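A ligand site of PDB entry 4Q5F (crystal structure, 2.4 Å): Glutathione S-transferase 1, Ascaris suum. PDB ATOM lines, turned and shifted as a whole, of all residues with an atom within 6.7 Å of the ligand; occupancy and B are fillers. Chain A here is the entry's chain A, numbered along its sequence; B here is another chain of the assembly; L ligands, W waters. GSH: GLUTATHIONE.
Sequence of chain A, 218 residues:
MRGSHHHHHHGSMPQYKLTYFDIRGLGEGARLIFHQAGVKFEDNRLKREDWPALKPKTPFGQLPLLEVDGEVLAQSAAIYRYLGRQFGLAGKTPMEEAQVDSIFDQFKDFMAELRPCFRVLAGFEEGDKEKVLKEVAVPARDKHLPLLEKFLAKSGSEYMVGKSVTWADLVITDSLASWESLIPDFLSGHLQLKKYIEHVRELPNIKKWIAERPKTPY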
ATOM      1  N   TYR A  20     -17.112  -2.396 -10.974  1.00  0.00           N
ATOM      2  CA  TYR A  20     -17.336  -2.909 -12.318  1.00  0.00           C
ATOM      3  C   TYR A  20     -18.647  -2.324 -12.831  1.00  0.00           C
ATOM      4  O   TYR A  20     -19.283  -1.545 -12.129  1.00  0.00           O
ATOM      5  CB  TYR A  20     -17.369  -4.441 -12.313  1.00  0.00           C
ATOM      6  CG  TYR A  20     -17.341  -5.072 -13.681  1.00  0.00           C
ATOM      7  CD1 TYR A  20     -16.234  -4.939 -14.515  1.00  0.00           C
ATOM      8  CD2 TYR A  20     -18.420  -5.800 -14.162  1.00  0.00           C
ATOM      9  CE1 TYR A  20     -16.207  -5.500 -15.777  1.00  0.00           C
ATOM     10  CE2 TYR A  20     -18.407  -6.378 -15.422  1.00  0.00           C
ATOM     11  CZ  TYR A  20     -17.293  -6.225 -16.221  1.00  0.00           C
ATOM     12  OH  TYR A  20     -17.273  -6.797 -17.477  1.00  0.00           O
ATOM     13  N   PHE A  21     -19.034  -2.669 -14.052  1.00  0.00           N
ATOM     14  CA  PHE A  21     -20.288  -2.184 -14.618  1.00  0.00           C
ATOM     15  C   PHE A  21     -21.478  -3.011 -14.149  1.00  0.00           C
ATOM     16  O   PHE A  21     -21.317  -3.980 -13.413  1.00  0.00           O
ATOM     17  CB  PHE A  21     -20.197  -2.171 -16.142  1.00  0.00           C
ATOM     18  CG  PHE A  21     -19.062  -1.338 -16.678  1.00  0.00           C
ATOM     19  CD1 PHE A  21     -19.084   0.042 -16.540  1.00  0.00           C
ATOM     20  CD2 PHE A  21     -17.986  -1.937 -17.301  1.00  0.00           C
ATOM     21  CE1 PHE A  21     -18.043   0.811 -17.034  1.00  0.00           C
ATOM     22  CE2 PHE A  21     -16.938  -1.162 -17.791  1.00  0.00           C
ATOM     23  CZ  PHE A  21     -16.967   0.207 -17.649  1.00  0.00           C
ATOM     24  N   ILE A  23     -23.395  -5.065 -15.642  1.00  0.00           N
ATOM     25  CA  ILE A  23     -23.472  -6.418 -16.190  1.00  0.00           C
ATOM     26  C   ILE A  23     -22.561  -7.395 -15.449  1.00  0.00           C
ATOM     27  O   ILE A  23     -21.727  -6.998 -14.645  1.00  0.00           O
ATOM     28  CB  ILE A  23     -23.126  -6.419 -17.692  1.00  0.00           C
ATOM     29  CG1 ILE A  23     -21.719  -5.862 -17.938  1.00  0.00           C
ATOM     30  CG2 ILE A  23     -24.167  -5.617 -18.465  1.00  0.00           C
ATOM     31  CD1 ILE A  23     -20.645  -6.918 -18.061  1.00  0.00           C
ATOM     32  N   GLY A  25     -20.330 -10.021 -16.893  1.00  0.00           N
ATOM     33  CA  GLY A  25     -19.043  -9.915 -17.566  1.00  0.00           C
ATOM     34  C   GLY A  25     -17.878 -10.486 -16.786  1.00  0.00           C
ATOM     35  O   GLY A  25     -17.927 -11.625 -16.323  1.00  0.00           O
ATOM     36  N   LEU A  26     -16.828  -9.689 -16.646  1.00  0.00           N
ATOM     37  CA  LEU A  26     -15.617 -10.106 -15.940  1.00  0.00           C
ATOM     38  C   LEU A  26     -15.740  -9.923 -14.434  1.00  0.00           C
ATOM     39  O   LEU A  26     -15.030 -10.580 -13.670  1.00  0.00           O
ATOM     40  CB  LEU A  26     -14.420  -9.312 -16.451  1.00  0.00           C
ATOM     41  CG  LEU A  26     -13.988  -9.564 -17.895  1.00  0.00           C
ATOM     42  CD1 LEU A  26     -12.827  -8.657 -18.274  1.00  0.00           C
ATOM     43  CD2 LEU A  26     -13.619 -11.023 -18.112  1.00  0.00           C
ATOM     44  N   TRP A  51     -17.978   6.670 -15.960  1.00  0.00           N
ATOM     45  CA  TRP A  51     -16.784   6.000 -16.472  1.00  0.00           C
ATOM     46  C   TRP A  51     -15.705   6.956 -16.997  1.00  0.00           C
ATOM     47  O   TRP A  51     -14.518   6.703 -16.774  1.00  0.00           O
ATOM     48  CB  TRP A  51     -17.157   4.973 -17.545  1.00  0.00           C
ATOM     49  CG  TRP A  51     -15.972   4.208 -18.075  1.00  0.00           C
ATOM     50  CD1 TRP A  51     -15.677   3.956 -19.386  1.00  0.00           C
ATOM     51  CD2 TRP A  51     -14.928   3.603 -17.307  1.00  0.00           C
ATOM     52  NE1 TRP A  51     -14.513   3.239 -19.478  1.00  0.00           N
ATOM     53  CE2 TRP A  51     -14.030   3.005 -18.221  1.00  0.00           C
ATOM     54  CE3 TRP A  51     -14.651   3.509 -15.932  1.00  0.00           C
ATOM     55  CZ2 TRP A  51     -12.883   2.320 -17.803  1.00  0.00           C
ATOM     56  CZ3 TRP A  51     -13.516   2.834 -15.532  1.00  0.00           C
ATOM     57  CH2 TRP A  51     -12.654   2.252 -16.461  1.00  0.00           C
ATOM     58  N   LYS A  55     -11.951   6.426 -15.449  1.00  0.00           N
ATOM     59  CA  LYS A  55     -11.020   5.725 -16.339  1.00  0.00           C
ATOM     60  C   LYS A  55      -9.558   6.147 -16.213  1.00  0.00           C
ATOM     61  O   LYS A  55      -8.676   5.297 -16.078  1.00  0.00           O
ATOM     62  CB  LYS A  55     -11.479   5.867 -17.796  1.00  0.00           C
ATOM     63  CG  LYS A  55     -10.653   5.092 -18.799  1.00  0.00           C
ATOM     64  CD  LYS A  55     -11.212   5.253 -20.201  1.00  0.00           C
ATOM     65  CE  LYS A  55     -10.268   4.707 -21.268  1.00  0.00           C
ATOM     66  NZ  LYS A  55     -10.347   3.230 -21.405  1.00  0.00           N
ATOM     67  N   PHE A  60      -4.989   0.636 -15.454  1.00  0.00           N
ATOM     68  CA  PHE A  60      -4.856   0.294 -16.877  1.00  0.00           C
ATOM     69  C   PHE A  60      -6.005   0.852 -17.720  1.00  0.00           C
ATOM     70  O   PHE A  60      -6.131   0.523 -18.902  1.00  0.00           O
ATOM     71  CB  PHE A  60      -4.794  -1.225 -17.056  1.00  0.00           C
ATOM     72  CG  PHE A  60      -3.731  -1.888 -16.227  1.00  0.00           C
ATOM     73  CD1 PHE A  60      -2.428  -1.406 -16.221  1.00  0.00           C
ATOM     74  CD2 PHE A  60      -4.032  -2.995 -15.455  1.00  0.00           C
ATOM     75  CE1 PHE A  60      -1.455  -2.022 -15.461  1.00  0.00           C
ATOM     76  CE2 PHE A  60      -3.067  -3.621 -14.689  1.00  0.00           C
ATOM     77  CZ  PHE A  60      -1.771  -3.129 -14.689  1.00  0.00           C
ATOM     78  N   GLY A  61      -6.851   1.688 -17.118  1.00  0.00           N
ATOM     79  CA  GLY A  61      -7.931   2.314 -17.853  1.00  0.00           C
ATOM     80  C   GLY A  61      -9.138   1.404 -18.049  1.00  0.00           C
ATOM     81  O   GLY A  61      -9.952   1.648 -18.943  1.00  0.00           O
ATOM     82  N   GLN A  62      -9.248   0.369 -17.220  1.00  0.00           N
ATOM     83  CA  GLN A  62     -10.309  -0.614 -17.360  1.00  0.00           C
ATOM     84  C   GLN A  62     -10.831  -1.150 -16.025  1.00  0.00           C
ATOM     85  O   GLN A  62     -10.176  -1.040 -14.996  1.00  0.00           O
ATOM     86  CB  GLN A  62      -9.853  -1.786 -18.240  1.00  0.00           C
ATOM     87  CG  GLN A  62      -9.580  -1.437 -19.686  1.00  0.00           C
ATOM     88  CD  GLN A  62      -9.394  -2.657 -20.565  1.00  0.00           C
ATOM     89  OE1 GLN A  62      -8.565  -3.513 -20.286  1.00  0.00           O
ATOM     90  NE2 GLN A  62     -10.175  -2.728 -21.634  1.00  0.00           N
ATOM     91  N   LEU A  63     -12.028  -1.731 -16.072  1.00  0.00           N
ATOM     92  CA  LEU A  63     -12.612  -2.427 -14.930  1.00  0.00           C
ATOM     93  C   LEU A  63     -12.575  -3.927 -15.259  1.00  0.00           C
ATOM     94  O   LEU A  63     -12.468  -4.305 -16.428  1.00  0.00           O
ATOM     95  CB  LEU A  63     -14.044  -1.934 -14.707  1.00  0.00           C
ATOM     96  CG  LEU A  63     -14.178  -0.431 -14.470  1.00  0.00           C
ATOM     97  CD1 LEU A  63     -15.639  -0.037 -14.303  1.00  0.00           C
ATOM     98  CD2 LEU A  63     -13.365   0.011 -13.252  1.00  0.00           C
ATOM     99  N   PRO A  64     -12.679  -4.790 -14.231  1.00  0.00           N
ATOM    100  CA  PRO A  64     -12.969  -4.499 -12.830  1.00  0.00           C
ATOM    101  C   PRO A  64     -11.766  -4.045 -12.018  1.00  0.00           C
ATOM    102  O   PRO A  64     -10.616  -4.227 -12.431  1.00  0.00           O
ATOM    103  CB  PRO A  64     -13.460  -5.832 -12.303  1.00  0.00           C
ATOM    104  CG  PRO A  64     -12.685  -6.836 -13.069  1.00  0.00           C
ATOM    105  CD  PRO A  64     -12.466  -6.234 -14.445  1.00  0.00           C
ATOM    106  N   ALA A  74      -6.043  -4.351 -10.038  1.00  0.00           N
ATOM    107  CA  ALA A  74      -6.678  -4.452 -11.348  1.00  0.00           C
ATOM    108  C   ALA A  74      -6.529  -5.858 -11.920  1.00  0.00           C
ATOM    109  O   ALA A  74      -5.883  -6.723 -11.318  1.00  0.00           O
ATOM    110  CB  ALA A  74      -6.063  -3.423 -12.304  1.00  0.00           C
ATOM    111  N   GLN A  75      -7.162  -6.082 -13.081  1.00  0.00           N
ATOM    112  CA  GLN A  75      -7.107  -7.353 -13.808  1.00  0.00           C
ATOM    113  C   GLN A  75      -7.902  -8.467 -13.134  1.00  0.00           C
ATOM    114  O   GLN A  75      -7.555  -8.944 -12.062  1.00  0.00           O
ATOM    115  CB  GLN A  75      -5.660  -7.792 -14.070  1.00  0.00           C
ATOM    116  CG  GLN A  75      -4.912  -6.894 -15.038  1.00  0.00           C
ATOM    117  CD  GLN A  75      -5.342  -7.094 -16.477  1.00  0.00           C
ATOM    118  OE1 GLN A  75      -6.116  -8.001 -16.785  1.00  0.00           O
ATOM    119  NE2 GLN A  75      -4.852  -6.236 -17.371  1.00  0.00           N
ATOM    120  N   SER A  76      -8.979  -8.868 -13.810  1.00  0.00           N
ATOM    121  CA  SER A  76      -9.953  -9.838 -13.277  1.00  0.00           C
ATOM    122  C   SER A  76      -9.319 -11.115 -12.734  1.00  0.00           C
ATOM    123  O   SER A  76      -9.637 -11.546 -11.620  1.00  0.00           O
ATOM    124  CB  SER A  76     -10.979 -10.191 -14.360  1.00  0.00           C
ATOM    125  OG  SER A  76     -10.345 -10.739 -15.506  1.00  0.00           O
ATOM    126  N   ALA A  77      -8.453 -11.751 -13.521  1.00  0.00           N
ATOM    127  CA  ALA A  77      -7.859 -13.019 -13.111  1.00  0.00           C
ATOM    128  C   ALA A  77      -7.017 -12.864 -11.857  1.00  0.00           C
ATOM    129  O   ALA A  77      -7.005 -13.735 -10.990  1.00  0.00           O
ATOM    130  CB  ALA A  77      -7.028 -13.605 -14.249  1.00  0.00           C
ATOM    131  N   ILE A  79      -7.593 -10.703  -9.641  1.00  0.00           N
ATOM    132  CA  ILE A  79      -8.592 -10.485  -8.609  1.00  0.00           C
ATOM    133  C   ILE A  79      -9.188 -11.818  -8.154  1.00  0.00           C
ATOM    134  O   ILE A  79      -9.370 -12.045  -6.958  1.00  0.00           O
ATOM    135  CB  ILE A  79      -9.713  -9.529  -9.093  1.00  0.00           C
ATOM    136  CG1 ILE A  79      -9.156  -8.109  -9.193  1.00  0.00           C
ATOM    137  CG2 ILE A  79     -10.904  -9.561  -8.148  1.00  0.00           C
ATOM    138  CD1 ILE A  79     -10.082  -7.127  -9.885  1.00  0.00           C
ATOM    139  N   TYR A  80      -9.476 -12.700  -9.110  1.00  0.00           N
ATOM    140  CA  TYR A  80     -10.021 -14.020  -8.783  1.00  0.00           C
ATOM    141  C   TYR A  80      -9.067 -14.769  -7.869  1.00  0.00           C
ATOM    142  O   TYR A  80      -9.470 -15.281  -6.813  1.00  0.00           O
ATOM    143  CB  TYR A  80     -10.217 -14.861 -10.046  1.00  0.00           C
ATOM    144  CG  TYR A  80     -11.107 -14.263 -11.111  1.00  0.00           C
ATOM    145  CD1 TYR A  80     -12.022 -13.266 -10.811  1.00  0.00           C
ATOM    146  CD2 TYR A  80     -11.041 -14.720 -12.428  1.00  0.00           C
ATOM    147  CE1 TYR A  80     -12.837 -12.719 -11.800  1.00  0.00           C
ATOM    148  CE2 TYR A  80     -11.849 -14.184 -13.411  1.00  0.00           C
ATOM    149  CZ  TYR A  80     -12.743 -13.191 -13.090  1.00  0.00           C
ATOM    150  OH  TYR A  80     -13.551 -12.668 -14.080  1.00  0.00           O
ATOM    151  N   LYS A 108      -9.388 -19.374 -20.521  1.00  0.00           N
ATOM    152  CA  LYS A 108      -9.249 -18.037 -21.078  1.00  0.00           C
ATOM    153  C   LYS A 108      -8.891 -18.094 -22.565  1.00  0.00           C
ATOM    154  O   LYS A 108      -9.315 -17.253 -23.345  1.00  0.00           O
ATOM    155  CB  LYS A 108      -8.203 -17.225 -20.311  1.00  0.00           C
ATOM    156  CG  LYS A 108      -8.758 -16.528 -19.070  1.00  0.00           C
ATOM    157  CD  LYS A 108      -7.763 -15.555 -18.444  1.00  0.00           C
ATOM    158  CE  LYS A 108      -7.784 -14.186 -19.103  1.00  0.00           C
ATOM    159  NZ  LYS A 108      -7.309 -13.108 -18.181  1.00  0.00           N
ATOM    160  N   ASP B 105      -0.705  -9.709 -16.429  1.00  0.00           N
ATOM    161  CA  ASP B 105      -1.953  -9.870 -17.172  1.00  0.00           C
ATOM    162  C   ASP B 105      -2.149  -8.725 -18.166  1.00  0.00           C
ATOM    163  O   ASP B 105      -2.677  -8.920 -19.250  1.00  0.00           O
ATOM    164  CB  ASP B 105      -3.160  -9.937 -16.223  1.00  0.00           C
ATOM    165  CG  ASP B 105      -3.371 -11.321 -15.637  1.00  0.00           C
ATOM    166  OD1 ASP B 105      -2.658 -12.272 -16.031  1.00  0.00           O
ATOM    167  OD2 ASP B 105      -4.273 -11.473 -14.785  1.00  0.00           O
ATOM    168  N   GLN B 106      -1.726  -7.523 -17.772  1.00  0.00           N
ATOM    169  CA  GLN B 106      -1.817  -6.376 -18.670  1.00  0.00           C
ATOM    170  C   GLN B 106      -0.816  -6.548 -19.814  1.00  0.00           C
ATOM    171  O   GLN B 106      -1.115  -6.226 -20.970  1.00  0.00           O
ATOM    172  CB  GLN B 106      -1.540  -5.075 -17.928  1.00  0.00           C
ATOM    173  CG  GLN B 106      -1.708  -3.824 -18.793  1.00  0.00           C
ATOM    174  CD  GLN B 106      -3.103  -3.677 -19.345  1.00  0.00           C
ATOM    175  OE1 GLN B 106      -4.077  -4.140 -18.748  1.00  0.00           O
ATOM    176  NE2 GLN B 106      -3.219  -3.035 -20.513  1.00  0.00           N
ATOM    177  N   ASP B 109      -2.390  -8.871 -22.179  1.00  0.00           N
ATOM    178  CA  ASP B 109      -3.353  -8.198 -23.056  1.00  0.00           C
ATOM    179  C   ASP B 109      -2.627  -7.525 -24.218  1.00  0.00           C
ATOM    180  O   ASP B 109      -3.067  -7.605 -25.362  1.00  0.00           O
ATOM    181  CB  ASP B 109      -4.148  -7.141 -22.284  1.00  0.00           C
ATOM    182  CG  ASP B 109      -5.200  -7.731 -21.371  1.00  0.00           C
ATOM    183  OD1 ASP B 109      -5.508  -8.937 -21.512  1.00  0.00           O
ATOM    184  OD2 ASP B 109      -5.727  -6.990 -20.515  1.00  0.00           O
ATOM    185  N   LYS B 143      -0.889   2.338 -26.973  1.00  0.00           N
ATOM    186  CA  LYS B 143      -1.852   2.196 -25.877  1.00  0.00           C
ATOM    187  C   LYS B 143      -1.220   1.569 -24.640  1.00  0.00           C
ATOM    188  O   LYS B 143      -1.438   2.042 -23.524  1.00  0.00           O
ATOM    189  CB  LYS B 143      -3.047   1.342 -26.304  1.00  0.00           C
ATOM    190  CG  LYS B 143      -4.183   1.363 -25.282  1.00  0.00           C
ATOM    191  CD  LYS B 143      -5.223   0.273 -25.505  1.00  0.00           C
ATOM    192  CE  LYS B 143      -6.524   0.619 -24.788  1.00  0.00           C
ATOM    193  NZ  LYS B 143      -7.404  -0.567 -24.579  1.00  0.00           N
HETATM  194  N1  GSH L   1      -7.670  -7.871 -19.125  1.00  0.00           N
HETATM  195  CA1 GSH L   1      -8.646  -7.130 -18.408  1.00  0.00           C
HETATM  196  C1  GSH L   1      -9.177  -7.972 -17.266  1.00  0.00           C
HETATM  197  O11 GSH L   1      -9.582  -7.421 -16.215  1.00  0.00           O
HETATM  198  O12 GSH L   1      -9.203  -9.220 -17.365  1.00  0.00           O
HETATM  199  CB1 GSH L   1      -9.776  -6.764 -19.358  1.00  0.00           C
HETATM  200  CG1 GSH L   1     -10.712  -5.762 -18.689  1.00  0.00           C
HETATM  201  CD1 GSH L   1     -11.687  -5.170 -19.714  1.00  0.00           C
HETATM  202  OE1 GSH L   1     -11.586  -5.460 -20.880  1.00  0.00           O
HETATM  203  N2  GSH L   1     -12.713  -4.265 -19.262  1.00  0.00           N
HETATM  204  CA2 GSH L   1     -13.648  -3.672 -20.172  1.00  0.00           C
HETATM  205  C2  GSH L   1     -13.620  -2.168 -19.952  1.00  0.00           C
HETATM  206  O2  GSH L   1     -13.136  -1.723 -18.925  1.00  0.00           O
HETATM  207  CB2 GSH L   1     -15.041  -4.174 -19.906  1.00  0.00           C
HETATM  208  SG2 GSH L   1     -15.083  -5.940 -20.019  1.00  0.00           S
HETATM  209  N3  GSH L   1     -14.159  -1.265 -20.942  1.00  0.00           N
HETATM  210  CA3 GSH L   1     -14.118   0.162 -20.731  1.00  0.00           C
HETATM  211  C3  GSH L   1     -12.777   0.718 -21.209  1.00  0.00           C
HETATM  212  O31 GSH L   1     -11.817  -0.052 -21.450  1.00  0.00           O
HETATM  213  O32 GSH L   1     -12.640   1.961 -21.350  1.00  0.00           O
HETATM  214  O   HOH W   1      -9.276  -5.027 -14.864  1.00  0.00           O
HETATM  215  O   HOH W   2      -9.938   0.396 -23.210  1.00  0.00           O
HETATM  216  O   HOH W   3      -6.981 -10.951 -15.909  1.00  0.00           O
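Water W2 lies within hydrogen-bond range of an oxygen (O31) of the ligand (2.6 Å), the side-chain amino group (NZ) of Lys 143 of chain B (3.0 Å) and the side-chain amino group (NZ) of Lys 55 (3.4 Å).
Water W1 lies within hydrogen-bond range of O11 of the ligand (2.8 Å), O of Pro 64 (2.9 Å) and N of Gln 75 (3.0 Å).
Water W3 lies within hydrogen-bond range of the backbone NH of Ala 77, the side-chain carboxylate of Asp 105 of chain B, the side-chain amino group of Lys 108, an oxygen (O12) of the ligand, the side-chain amide oxygen of Gln 75 and the side-chain hydroxyl of Ser 76.
OH of Tyr 80 lies within hydrogen-bond range of O of Leu 26, 2.6 Å away.
NE2 of Gln 75 is in hydrogen-bond range of OE1 of Gln 106 of chain B (2.6 Å).
The side-chain hydroxyl (OH) of Tyr 20 is in hydrogen-bond range of the backbone NH (N) of Leu 26.
The side-chain carboxylate (OD2) of Asp 109 of chain B is in hydrogen-bond range of the side-chain amide nitrogen (NE2) of Gln 75, at 3.3 Å.
The side-chain amino group of Lys 55 is in hydrogen-bond range of the backbone carbonyl oxygen of Gly 61.
N of Ser 76 lies within hydrogen-bond range of O11 of the ligand (2.9 Å).
A nitrogen (N1) of the ligand is in salt-bridge range of the side-chain carboxylate (OD2) of Asp 109 of chain B (2.5 Å).
An oxygen (O32) of the ligand sits at hydrogen-bond distance from the indole nitrogen (NE1) of Trp 51 (2.9 Å).
The side-chain amide oxygen (OE1) of Gln 75 sits at hydrogen-bond distance from a nitrogen (N1) of the ligand, 2.8 Å away.
The side-chain hydroxyl (OH) of Tyr 20 sits close to a sulfur (SG2) of the ligand (3.5 Å).
The backbone NH (N) of Leu 63 lies within hydrogen-bond range of an oxygen (O2) of the ligand (3.1 Å).
The side-chain hydroxyl (OG) of Ser 76 sits at hydrogen-bond distance from an oxygen (O12) of the ligand (2.7 Å).
The backbone carbonyl oxygen (O) of Leu 63 sits at hydrogen-bond distance from a nitrogen (N2) of the ligand, at 2.8 Å.
NZ of Lys 55 lies within salt-bridge range of O32 of the ligand.
The side-chain amide nitrogen of Gln 62 sits at hydrogen-bond distance from an oxygen (O31) of the ligand (3.1 Å).
Residues that only touch the ligand: Leu 26, Gly 61 and Pro 64.
Hydrophobic or aromatic side chains within 4 Å of the ligand: Leu 26, Trp 51 and Pro 64.
11 residues have an atom within 4 Å of the ligand: Tyr 20, Leu 26, Trp 51, Lys 55, Gly 61, Gln 62, Leu 63, Pro 64, Gln 75, Ser 76 and Asp 109 of chain B.
The nearest printed residue that does not touch the ligand is Phe 21 (4.01 Å).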
